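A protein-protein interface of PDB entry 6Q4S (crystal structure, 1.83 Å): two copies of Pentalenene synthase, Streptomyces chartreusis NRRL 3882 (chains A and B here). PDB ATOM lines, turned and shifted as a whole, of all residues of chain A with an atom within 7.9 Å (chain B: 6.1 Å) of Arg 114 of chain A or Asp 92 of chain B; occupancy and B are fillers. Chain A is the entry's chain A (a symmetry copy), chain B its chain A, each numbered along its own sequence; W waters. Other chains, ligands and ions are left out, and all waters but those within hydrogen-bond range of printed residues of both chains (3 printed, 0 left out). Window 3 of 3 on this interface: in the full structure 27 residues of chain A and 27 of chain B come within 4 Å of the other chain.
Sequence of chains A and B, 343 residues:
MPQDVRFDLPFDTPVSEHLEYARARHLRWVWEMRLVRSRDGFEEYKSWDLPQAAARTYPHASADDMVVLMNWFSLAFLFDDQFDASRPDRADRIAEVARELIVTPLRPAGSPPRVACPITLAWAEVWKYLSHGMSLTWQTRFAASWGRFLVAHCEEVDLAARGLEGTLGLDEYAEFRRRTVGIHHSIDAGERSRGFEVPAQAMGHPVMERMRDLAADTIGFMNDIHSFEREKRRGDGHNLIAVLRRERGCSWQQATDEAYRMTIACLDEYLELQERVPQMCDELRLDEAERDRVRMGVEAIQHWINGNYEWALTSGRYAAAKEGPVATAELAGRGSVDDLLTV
CG2 of Val 103 of chain A touches NH2 of Arg 99 of chain B (3.7 Å). Arg 99 of chain B touches Arg 107 of chain A (NH2 to NH2, 3.7 Å). Ala 91 of chain B touches Arg 114 of chain A. Ala 95 of chain B touches Arg 114 of chain A. Arg 99 of chain B touches Arg 114 of chain A.
The side-chain carboxylate (OD1) of Asp 92 of chain B is in salt-bridge range of the guanidinium group (NH2) of Arg 114 of chain A, 2.8 Å away. The guanidinium group of Arg 99 of chain B lies within salt-bridge range of the side-chain carboxylate of Glu 100 of chain A, 2.8 Å away. The side-chain carboxylate of Asp 158 of chain B is in salt-bridge range of the guanidinium group of Arg 114 of chain A (2.9 Å).
Of the printed residues of chain B, Glu 100 of chain A touches Arg 99 (2.8 Å). Of the printed residues of chain B, Val 103 of chain A touches Arg 99. Of the printed residues of chain B, Arg 114 of chain A touches Ala 91 (3.6 Å), Asp 92 (2.8 Å), Ala 95 (3.8 Å), Arg 99 (3.6 Å) and Asp 158 (2.9 Å). Ala 91 of chain B touches just one residue of chain A: Arg 114. Asp 92 of chain B touches just one residue of chain A: Arg 114. Printed residues of chain A within 4 Å of Ala 95 of chain B: Arg 114 (3.8 Å). Cys 154 of chain B touches none of the printed residues of chain A. The nearest printed residue of chain B that does not touch Arg 114 of chain A is Cys 154 of chain B (5.4 Å). The nearest residue of chain A that does not touch Asp 92 of chain B is Glu 96 of chain A (7.4 Å).
Hydrophobic or aromatic side chains of chain A within 4 Å of the printed part of chain B: Val 103. Along chain A the printed residues that touch a printed residue of chain B span positions 100 to 114. Among the printed residues, 8 pairs touch across the chains. Among the printed residues, Asp or Glu carboxylates within 4 Å of a Lys or Arg side-chain nitrogen of the other chain: Glu 100 of chain A with Arg 99 of chain B, Arg 114 of chain A with Asp 92 of chain B and Arg 114 of chain A with Asp 158 of chain B.
Water W1 bridges NH1 of Arg 99 of chain B and O of Glu 96 of chain A. Water W3 bridges the backbone carbonyl oxygen of Asp 92 of chain B (2.7 Å) and the guanidinium group of Arg 114 of chain A (3.5 Å). Water W2 lies within hydrogen-bond range of the guanidinium group (NH2) of Arg 99 of chain B (3.2 Å) and the guanidinium group (NH2) of Arg 107 of chain A (3.5 Å).
The side-chain hydroxyl of Thr 104 of chain A lies within hydrogen-bond range of the backbone carbonyl oxygen of Glu 100 of chain A (3.1 Å). The guanidinium group of Arg 107 of chain A lies within salt-bridge range of the side-chain carboxylate of Glu 100 of chain A, at 2.7 Å. The side-chain carboxylate (OE1) of Glu 100 of chain A sits at hydrogen-bond distance from the backbone NH (N) of Arg 114 of chain A (3.1 Å). The side-chain carboxylate of Glu 100 of chain A sits at hydrogen-bond distance from the backbone NH of Val 115 of chain A, 3.0 Å away. The side-chain hydroxyl (OG1) of Thr 104 of chain A lies within hydrogen-bond range of the guanidinium group (NH1) of Arg 107 of chain A (3.0 Å).
Position printed for both chains: 96. Of the 8 pairs that touch across the chains among the printed residues, none has its exchanged pair printed and touching as well.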
ATOM      1  N   GLU A  96     -22.424 -24.421 -36.682  1.00  0.00           N
ATOM      2  CA  GLU A  96     -22.733 -23.802 -35.427  1.00  0.00           C
ATOM      3  C   GLU A  96     -22.870 -24.805 -34.250  1.00  0.00           C
ATOM      4  O   GLU A  96     -22.325 -24.588 -33.146  1.00  0.00           O
ATOM      5  CB  GLU A  96     -23.966 -22.888 -35.557  1.00  0.00           C
ATOM      6  CG  GLU A  96     -24.390 -22.200 -34.290  1.00  0.00           C
ATOM      7  CD  GLU A  96     -25.573 -21.191 -34.404  1.00  0.00           C
ATOM      8  OE1 GLU A  96     -26.433 -21.264 -35.351  1.00  0.00           O
ATOM      9  OE2 GLU A  96     -25.630 -20.329 -33.476  1.00  0.00           O
ATOM     10  N   GLU A 100     -20.232 -25.902 -30.906  1.00  0.00           N
ATOM     11  CA  GLU A 100     -20.668 -26.019 -29.502  1.00  0.00           C
ATOM     12  C   GLU A 100     -20.216 -27.355 -28.967  1.00  0.00           C
ATOM     13  O   GLU A 100     -19.649 -27.438 -27.877  1.00  0.00           O
ATOM     14  CB  GLU A 100     -22.219 -25.849 -29.354  1.00  0.00           C
ATOM     15  CG  GLU A 100     -22.694 -25.885 -27.919  1.00  0.00           C
ATOM     16  CD  GLU A 100     -22.253 -24.671 -27.130  1.00  0.00           C
ATOM     17  OE1 GLU A 100     -21.717 -24.792 -26.008  1.00  0.00           O
ATOM     18  OE2 GLU A 100     -22.464 -23.543 -27.635  1.00  0.00           O
ATOM     19  N   VAL A 103     -16.468 -27.019 -28.148  1.00  0.00           N
ATOM     20  CA  VAL A 103     -16.001 -26.269 -26.969  1.00  0.00           C
ATOM     21  C   VAL A 103     -16.426 -26.895 -25.658  1.00  0.00           C
ATOM     22  O   VAL A 103     -15.895 -26.566 -24.647  1.00  0.00           O
ATOM     23  CB  VAL A 103     -16.412 -24.803 -27.018  1.00  0.00           C
ATOM     24  CG1 VAL A 103     -15.869 -24.137 -28.261  1.00  0.00           C
ATOM     25  CG2 VAL A 103     -17.889 -24.589 -27.013  1.00  0.00           C
ATOM     26  N   THR A 104     -17.364 -27.842 -25.668  1.00  0.00           N
ATOM     27  CA  THR A 104     -17.906 -28.417 -24.413  1.00  0.00           C
ATOM     28  C   THR A 104     -16.791 -29.069 -23.626  1.00  0.00           C
ATOM     29  O   THR A 104     -16.687 -28.850 -22.417  1.00  0.00           O
ATOM     30  CB  THR A 104     -19.116 -29.332 -24.732  1.00  0.00           C
ATOM     31  OG1 THR A 104     -20.231 -28.504 -25.072  1.00  0.00           O
ATOM     32  CG2 THR A 104     -19.487 -30.248 -23.604  1.00  0.00           C
ATOM     33  N   ARG A 107     -14.435 -26.485 -21.449  1.00  0.00           N
ATOM     34  CA  ARG A 107     -15.046 -25.645 -20.406  1.00  0.00           C
ATOM     35  C   ARG A 107     -15.364 -26.588 -19.193  1.00  0.00           C
ATOM     36  O   ARG A 107     -15.410 -27.807 -19.372  1.00  0.00           O
ATOM     37  CB  ARG A 107     -16.254 -24.944 -21.056  1.00  0.00           C
ATOM     38  CG  ARG A 107     -17.601 -25.302 -20.559  1.00  0.00           C
ATOM     39  CD  ARG A 107     -18.728 -25.466 -21.527  1.00  0.00           C
ATOM     40  NE  ARG A 107     -19.038 -24.406 -22.417  1.00  0.00           N
ATOM     41  CZ  ARG A 107     -19.815 -24.599 -23.475  1.00  0.00           C
ATOM     42  NH1 ARG A 107     -20.420 -25.779 -23.723  1.00  0.00           N
ATOM     43  NH2 ARG A 107     -20.008 -23.595 -24.291  1.00  0.00           N
ATOM     44  N   SER A 111     -21.007 -27.117 -17.001  1.00  0.00           N
ATOM     45  CA  SER A 111     -21.452 -25.910 -17.657  1.00  0.00           C
ATOM     46  C   SER A 111     -22.454 -26.113 -18.768  1.00  0.00           C
ATOM     47  O   SER A 111     -22.307 -27.017 -19.582  1.00  0.00           O
ATOM     48  CB  SER A 111     -20.276 -25.193 -18.303  1.00  0.00           C
ATOM     49  OG  SER A 111     -19.248 -25.014 -17.371  1.00  0.00           O
ATOM     50  N   PRO A 112     -23.425 -25.213 -18.870  1.00  0.00           N
ATOM     51  CA  PRO A 112     -24.420 -25.221 -19.915  1.00  0.00           C
ATOM     52  C   PRO A 112     -23.835 -24.757 -21.235  1.00  0.00           C
ATOM     53  O   PRO A 112     -22.968 -23.865 -21.249  1.00  0.00           O
ATOM     54  CB  PRO A 112     -25.437 -24.159 -19.466  1.00  0.00           C
ATOM     55  CG  PRO A 112     -24.652 -23.237 -18.620  1.00  0.00           C
ATOM     56  CD  PRO A 112     -23.563 -24.033 -17.995  1.00  0.00           C
ATOM     57  N   PRO A 113     -24.307 -25.341 -22.324  1.00  0.00           N
ATOM     58  CA  PRO A 113     -23.923 -24.903 -23.647  1.00  0.00           C
ATOM     59  C   PRO A 113     -24.559 -23.586 -24.030  1.00  0.00           C
ATOM     60  O   PRO A 113     -25.687 -23.321 -23.672  1.00  0.00           O
ATOM     61  CB  PRO A 113     -24.473 -25.987 -24.539  1.00  0.00           C
ATOM     62  CG  PRO A 113     -25.658 -26.500 -23.803  1.00  0.00           C
ATOM     63  CD  PRO A 113     -25.218 -26.500 -22.376  1.00  0.00           C
ATOM     64  N   ARG A 114     -23.880 -22.817 -24.869  1.00  0.00           N
ATOM     65  CA  ARG A 114     -24.381 -21.526 -25.302  1.00  0.00           C
ATOM     66  C   ARG A 114     -25.480 -21.674 -26.352  1.00  0.00           C
ATOM     67  O   ARG A 114     -26.465 -21.006 -26.299  1.00  0.00           O
ATOM     68  CB  ARG A 114     -23.184 -20.702 -25.857  1.00  0.00           C
ATOM     69  CG  ARG A 114     -23.415 -19.207 -25.981  1.00  0.00           C
ATOM     70  CD  ARG A 114     -22.136 -18.407 -26.374  1.00  0.00           C
ATOM     71  NE  ARG A 114     -22.371 -16.943 -26.305  1.00  0.00           N
ATOM     72  CZ  ARG A 114     -23.144 -16.235 -27.131  1.00  0.00           C
ATOM     73  NH1 ARG A 114     -23.707 -16.785 -28.197  1.00  0.00           N
ATOM     74  NH2 ARG A 114     -23.329 -14.915 -26.918  1.00  0.00           N
ATOM     75  N   VAL A 115     -25.233 -22.493 -27.353  1.00  0.00           N
ATOM     76  CA  VAL A 115     -26.226 -23.017 -28.307  1.00  0.00           C
ATOM     77  C   VAL A 115     -26.921 -24.242 -27.611  1.00  0.00           C
ATOM     78  O   VAL A 115     -26.292 -25.277 -27.445  1.00  0.00           O
ATOM     79  CB  VAL A 115     -25.481 -23.457 -29.576  1.00  0.00           C
ATOM     80  CG1 VAL A 115     -26.382 -24.083 -30.637  1.00  0.00           C
ATOM     81  CG2 VAL A 115     -24.767 -22.264 -30.195  1.00  0.00           C
ATOM     82  N   ALA A 116     -28.156 -24.069 -27.150  1.00  0.00           N
ATOM     83  CA  ALA A 116     -28.947 -25.123 -26.458  1.00  0.00           C
ATOM     84  C   ALA A 116     -29.889 -25.809 -27.438  1.00  0.00           C
ATOM     85  O   ALA A 116     -30.807 -25.198 -27.980  1.00  0.00           O
ATOM     86  CB  ALA A 116     -29.765 -24.519 -25.319  1.00  0.00           C
ATOM     87  N   CYS A 117     -29.608 -27.057 -27.748  1.00  0.00           N
ATOM     88  CA  CYS A 117     -30.526 -27.852 -28.531  1.00  0.00           C
ATOM     89  C   CYS A 117     -30.373 -29.248 -27.967  1.00  0.00           C
ATOM     90  O   CYS A 117     -29.502 -29.458 -27.130  1.00  0.00           O
ATOM     91  CB  CYS A 117     -30.246 -27.696 -30.024  1.00  0.00           C
ATOM     92  SG  CYS A 117     -28.702 -28.370 -30.650  1.00  0.00           S
ATOM     93  N   THR A 120     -26.726 -30.684 -27.950  1.00  0.00           N
ATOM     94  CA  THR A 120     -25.662 -29.981 -27.198  1.00  0.00           C
ATOM     95  C   THR A 120     -25.874 -30.197 -25.725  1.00  0.00           C
ATOM     96  O   THR A 120     -24.928 -30.376 -24.980  1.00  0.00           O
ATOM     97  CB  THR A 120     -25.544 -28.492 -27.560  1.00  0.00           C
ATOM     98  OG1 THR A 120     -26.758 -27.744 -27.293  1.00  0.00           O
ATOM     99  CG2 THR A 120     -25.191 -28.356 -29.017  1.00  0.00           C
ATOM    100  N   LEU A 121     -27.138 -30.231 -25.315  1.00  0.00           N
ATOM    101  CA  LEU A 121     -27.461 -30.578 -23.931  1.00  0.00           C
ATOM    102  C   LEU A 121     -27.096 -31.997 -23.591  1.00  0.00           C
ATOM    103  O   LEU A 121     -26.577 -32.240 -22.511  1.00  0.00           O
ATOM    104  CB  LEU A 121     -28.961 -30.332 -23.663  1.00  0.00           C
ATOM    105  CG  LEU A 121     -29.346 -28.835 -23.783  1.00  0.00           C
ATOM    106  CD1 LEU A 121     -30.852 -28.721 -24.062  1.00  0.00           C
ATOM    107  CD2 LEU A 121     -28.950 -28.020 -22.556  1.00  0.00           C
ATOM    108  N   ASP B  89     -26.196  -7.413 -30.984  1.00  0.00           N
ATOM    109  CA  ASP B  89     -25.748  -8.809 -30.814  1.00  0.00           C
ATOM    110  C   ASP B  89     -24.204  -8.942 -30.826  1.00  0.00           C
ATOM    111  O   ASP B  89     -23.660  -9.926 -31.351  1.00  0.00           O
ATOM    112  CB  ASP B  89     -26.346  -9.644 -31.956  1.00  0.00           C
ATOM    113  CG  ASP B  89     -25.867  -9.171 -33.339  1.00  0.00           C
ATOM    114  OD1 ASP B  89     -25.620  -7.943 -33.527  1.00  0.00           O
ATOM    115  OD2 ASP B  89     -25.714 -10.033 -34.220  1.00  0.00           O
ATOM    116  N   ARG B  90     -23.524  -7.942 -30.265  1.00  0.00           N
ATOM    117  CA  ARG B  90     -22.071  -7.898 -30.193  1.00  0.00           C
ATOM    118  C   ARG B  90     -21.527  -9.250 -29.631  1.00  0.00           C
ATOM    119  O   ARG B  90     -20.684  -9.892 -30.252  1.00  0.00           O
ATOM    120  CB  ARG B  90     -21.624  -6.733 -29.285  1.00  0.00           C
ATOM    121  CG  ARG B  90     -20.189  -6.297 -29.510  1.00  0.00           C
ATOM    122  CD  ARG B  90     -19.533  -5.606 -28.308  1.00  0.00           C
ATOM    123  NE  ARG B  90     -18.096  -5.472 -28.592  1.00  0.00           N
ATOM    124  CZ  ARG B  90     -17.087  -5.439 -27.710  1.00  0.00           C
ATOM    125  NH1 ARG B  90     -17.297  -5.485 -26.391  1.00  0.00           N
ATOM    126  NH2 ARG B  90     -15.831  -5.355 -28.180  1.00  0.00           N
ATOM    127  N   ALA B  91     -22.049  -9.637 -28.464  1.00  0.00           N
ATOM    128  CA  ALA B  91     -21.632 -10.824 -27.733  1.00  0.00           C
ATOM    129  C   ALA B  91     -21.762 -12.136 -28.568  1.00  0.00           C
ATOM    130  O   ALA B  91     -20.834 -12.946 -28.554  1.00  0.00           O
ATOM    131  CB  ALA B  91     -22.343 -10.917 -26.397  1.00  0.00           C
ATOM    132  N   ASP B  92     -22.806 -12.259 -29.389  1.00  0.00           N
ATOM    133  CA  ASP B  92     -22.960 -13.362 -30.354  1.00  0.00           C
ATOM    134  C   ASP B  92     -21.934 -13.338 -31.498  1.00  0.00           C
ATOM    135  O   ASP B  92     -21.434 -14.383 -31.900  1.00  0.00           O
ATOM    136  CB  ASP B  92     -24.349 -13.409 -31.007  1.00  0.00           C
ATOM    137  CG  ASP B  92     -25.477 -13.780 -30.048  1.00  0.00           C
ATOM    138  OD1 ASP B  92     -25.251 -14.238 -28.891  1.00  0.00           O
ATOM    139  OD2 ASP B  92     -26.637 -13.622 -30.496  1.00  0.00           O
ATOM    140  N   ARG B  93     -21.644 -12.171 -32.045  1.00  0.00           N
ATOM    141  CA  ARG B  93     -20.601 -12.084 -33.054  1.00  0.00           C
ATOM    142  C   ARG B  93     -19.223 -12.440 -32.456  1.00  0.00           C
ATOM    143  O   ARG B  93     -18.488 -13.156 -33.082  1.00  0.00           O
ATOM    144  CB  ARG B  93     -20.584 -10.712 -33.728  1.00  0.00           C
ATOM    145  CG  ARG B  93     -19.584 -10.596 -34.872  1.00  0.00           C
ATOM    146  CD  ARG B  93     -19.738 -11.668 -35.948  1.00  0.00           C
ATOM    147  NE  ARG B  93     -18.806 -11.436 -37.039  1.00  0.00           N
ATOM    148  CZ  ARG B  93     -18.752 -12.150 -38.153  1.00  0.00           C
ATOM    149  NH1 ARG B  93     -19.554 -13.191 -38.318  1.00  0.00           N
ATOM    150  NH2 ARG B  93     -17.867 -11.842 -39.106  1.00  0.00           N
ATOM    151  N   ILE B  94     -18.915 -11.985 -31.261  1.00  0.00           N
ATOM    152  CA  ILE B  94     -17.674 -12.347 -30.572  1.00  0.00           C
ATOM    153  C   ILE B  94     -17.543 -13.891 -30.397  1.00  0.00           C
ATOM    154  O   ILE B  94     -16.517 -14.462 -30.750  1.00  0.00           O
ATOM    155  CB  ILE B  94     -17.532 -11.555 -29.280  1.00  0.00           C
ATOM    156  CG1 ILE B  94     -17.148 -10.086 -29.629  1.00  0.00           C
ATOM    157  CG2 ILE B  94     -16.494 -12.145 -28.303  1.00  0.00           C
ATOM    158  CD1 ILE B  94     -17.242  -9.180 -28.425  1.00  0.00           C
ATOM    159  N   ALA B  95     -18.611 -14.556 -29.952  1.00  0.00           N
ATOM    160  CA  ALA B  95     -18.581 -15.988 -29.765  1.00  0.00           C
ATOM    161  C   ALA B  95     -18.327 -16.675 -31.025  1.00  0.00           C
ATOM    162  O   ALA B  95     -17.617 -17.679 -31.039  1.00  0.00           O
ATOM    163  CB  ALA B  95     -19.905 -16.516 -29.178  1.00  0.00           C
ATOM    164  N   GLU B  96     -18.971 -16.200 -32.094  1.00  0.00           N
ATOM    165  CA  GLU B  96     -18.789 -16.731 -33.412  1.00  0.00           C
ATOM    166  C   GLU B  96     -17.322 -16.659 -33.918  1.00  0.00           C
ATOM    167  O   GLU B  96     -16.781 -17.640 -34.473  1.00  0.00           O
ATOM    168  CB  GLU B  96     -19.776 -16.086 -34.403  1.00  0.00           C
ATOM    169  CG  GLU B  96     -19.658 -16.559 -35.824  1.00  0.00           C
ATOM    170  CD  GLU B  96     -20.706 -16.004 -36.836  1.00  0.00           C
ATOM    171  OE1 GLU B  96     -21.319 -14.897 -36.632  1.00  0.00           O
ATOM    172  OE2 GLU B  96     -20.870 -16.711 -37.876  1.00  0.00           O
ATOM    173  N   VAL B  97     -16.688 -15.505 -33.701  1.00  0.00           N
ATOM    174  CA  VAL B  97     -15.335 -15.313 -34.151  1.00  0.00           C
ATOM    175  C   VAL B  97     -14.371 -16.077 -33.267  1.00  0.00           C
ATOM    176  O   VAL B  97     -13.473 -16.724 -33.800  1.00  0.00           O
ATOM    177  CB  VAL B  97     -14.985 -13.793 -34.223  1.00  0.00           C
ATOM    178  CG1 VAL B  97     -13.503 -13.625 -34.522  1.00  0.00           C
ATOM    179  CG2 VAL B  97     -15.861 -13.152 -35.301  1.00  0.00           C
ATOM    180  N   ARG B  99     -14.875 -18.843 -31.713  1.00  0.00           N
ATOM    181  CA  ARG B  99     -14.935 -20.277 -32.091  1.00  0.00           C
ATOM    182  C   ARG B  99     -14.197 -20.594 -33.361  1.00  0.00           C
ATOM    183  O   ARG B  99     -13.683 -21.693 -33.486  1.00  0.00           O
ATOM    184  CB  ARG B  99     -16.395 -20.744 -32.185  1.00  0.00           C
ATOM    185  CG  ARG B  99     -16.980 -20.767 -30.786  1.00  0.00           C
ATOM    186  CD  ARG B  99     -18.429 -21.180 -30.663  1.00  0.00           C
ATOM    187  NE  ARG B  99     -18.831 -21.183 -29.245  1.00  0.00           N
ATOM    188  CZ  ARG B  99     -19.926 -21.802 -28.777  1.00  0.00           C
ATOM    189  NH1 ARG B  99     -20.739 -22.450 -29.610  1.00  0.00           N
ATOM    190  NH2 ARG B  99     -20.190 -21.774 -27.493  1.00  0.00           N
ATOM    191  N   CYS B 154     -15.190 -15.711 -23.959  1.00  0.00           N
ATOM    192  CA  CYS B 154     -16.630 -15.599 -24.313  1.00  0.00           C
ATOM    193  C   CYS B 154     -17.524 -15.543 -23.076  1.00  0.00           C
ATOM    194  O   CYS B 154     -18.507 -14.787 -23.075  1.00  0.00           O
ATOM    195  CB  CYS B 154     -17.075 -16.756 -25.234  1.00  0.00           C
ATOM    196  SG  CYS B 154     -16.278 -16.663 -26.842  1.00  0.00           S
ATOM    197  N   ASP B 158     -20.065 -12.429 -22.194  1.00  0.00           N
ATOM    198  CA  ASP B 158     -21.506 -12.631 -21.945  1.00  0.00           C
ATOM    199  C   ASP B 158     -21.875 -12.081 -20.565  1.00  0.00           C
ATOM    200  O   ASP B 158     -22.943 -11.513 -20.420  1.00  0.00           O
ATOM    201  CB  ASP B 158     -21.952 -14.109 -22.064  1.00  0.00           C
ATOM    202  CG  ASP B 158     -21.959 -14.630 -23.499  1.00  0.00           C
ATOM    203  OD1 ASP B 158     -22.332 -13.888 -24.452  1.00  0.00           O
ATOM    204  OD2 ASP B 158     -21.596 -15.834 -23.681  1.00  0.00           O
ATOM    205  N   ARG B 162     -24.739  -9.256 -20.184  1.00  0.00           N
ATOM    206  CA  ARG B 162     -25.948  -9.601 -19.409  1.00  0.00           C
ATOM    207  C   ARG B 162     -26.197  -8.757 -18.151  1.00  0.00           C
ATOM    208  O   ARG B 162     -27.202  -8.968 -17.461  1.00  0.00           O
ATOM    209  CB  ARG B 162     -25.899 -11.077 -19.006  1.00  0.00           C
ATOM    210  CG  ARG B 162     -26.145 -11.966 -20.215  1.00  0.00           C
ATOM    211  CD  ARG B 162     -25.772 -13.405 -19.876  1.00  0.00           C
ATOM    212  NE  ARG B 162     -25.926 -14.215 -21.086  1.00  0.00           N
ATOM    213  CZ  ARG B 162     -25.760 -15.535 -21.122  1.00  0.00           C
ATOM    214  NH1 ARG B 162     -25.488 -16.202 -20.025  1.00  0.00           N
ATOM    215  NH2 ARG B 162     -25.942 -16.189 -22.274  1.00  0.00           N
HETATM  216  O   HOH W   1     -21.164 -22.277 -32.196  1.00  0.00           O
HETATM  217  O   HOH W   2     -19.031 -20.324 -24.843  1.00  0.00           O
HETATM  218  O   HOH W   3     -22.633 -16.817 -31.517  1.00  0.00           O
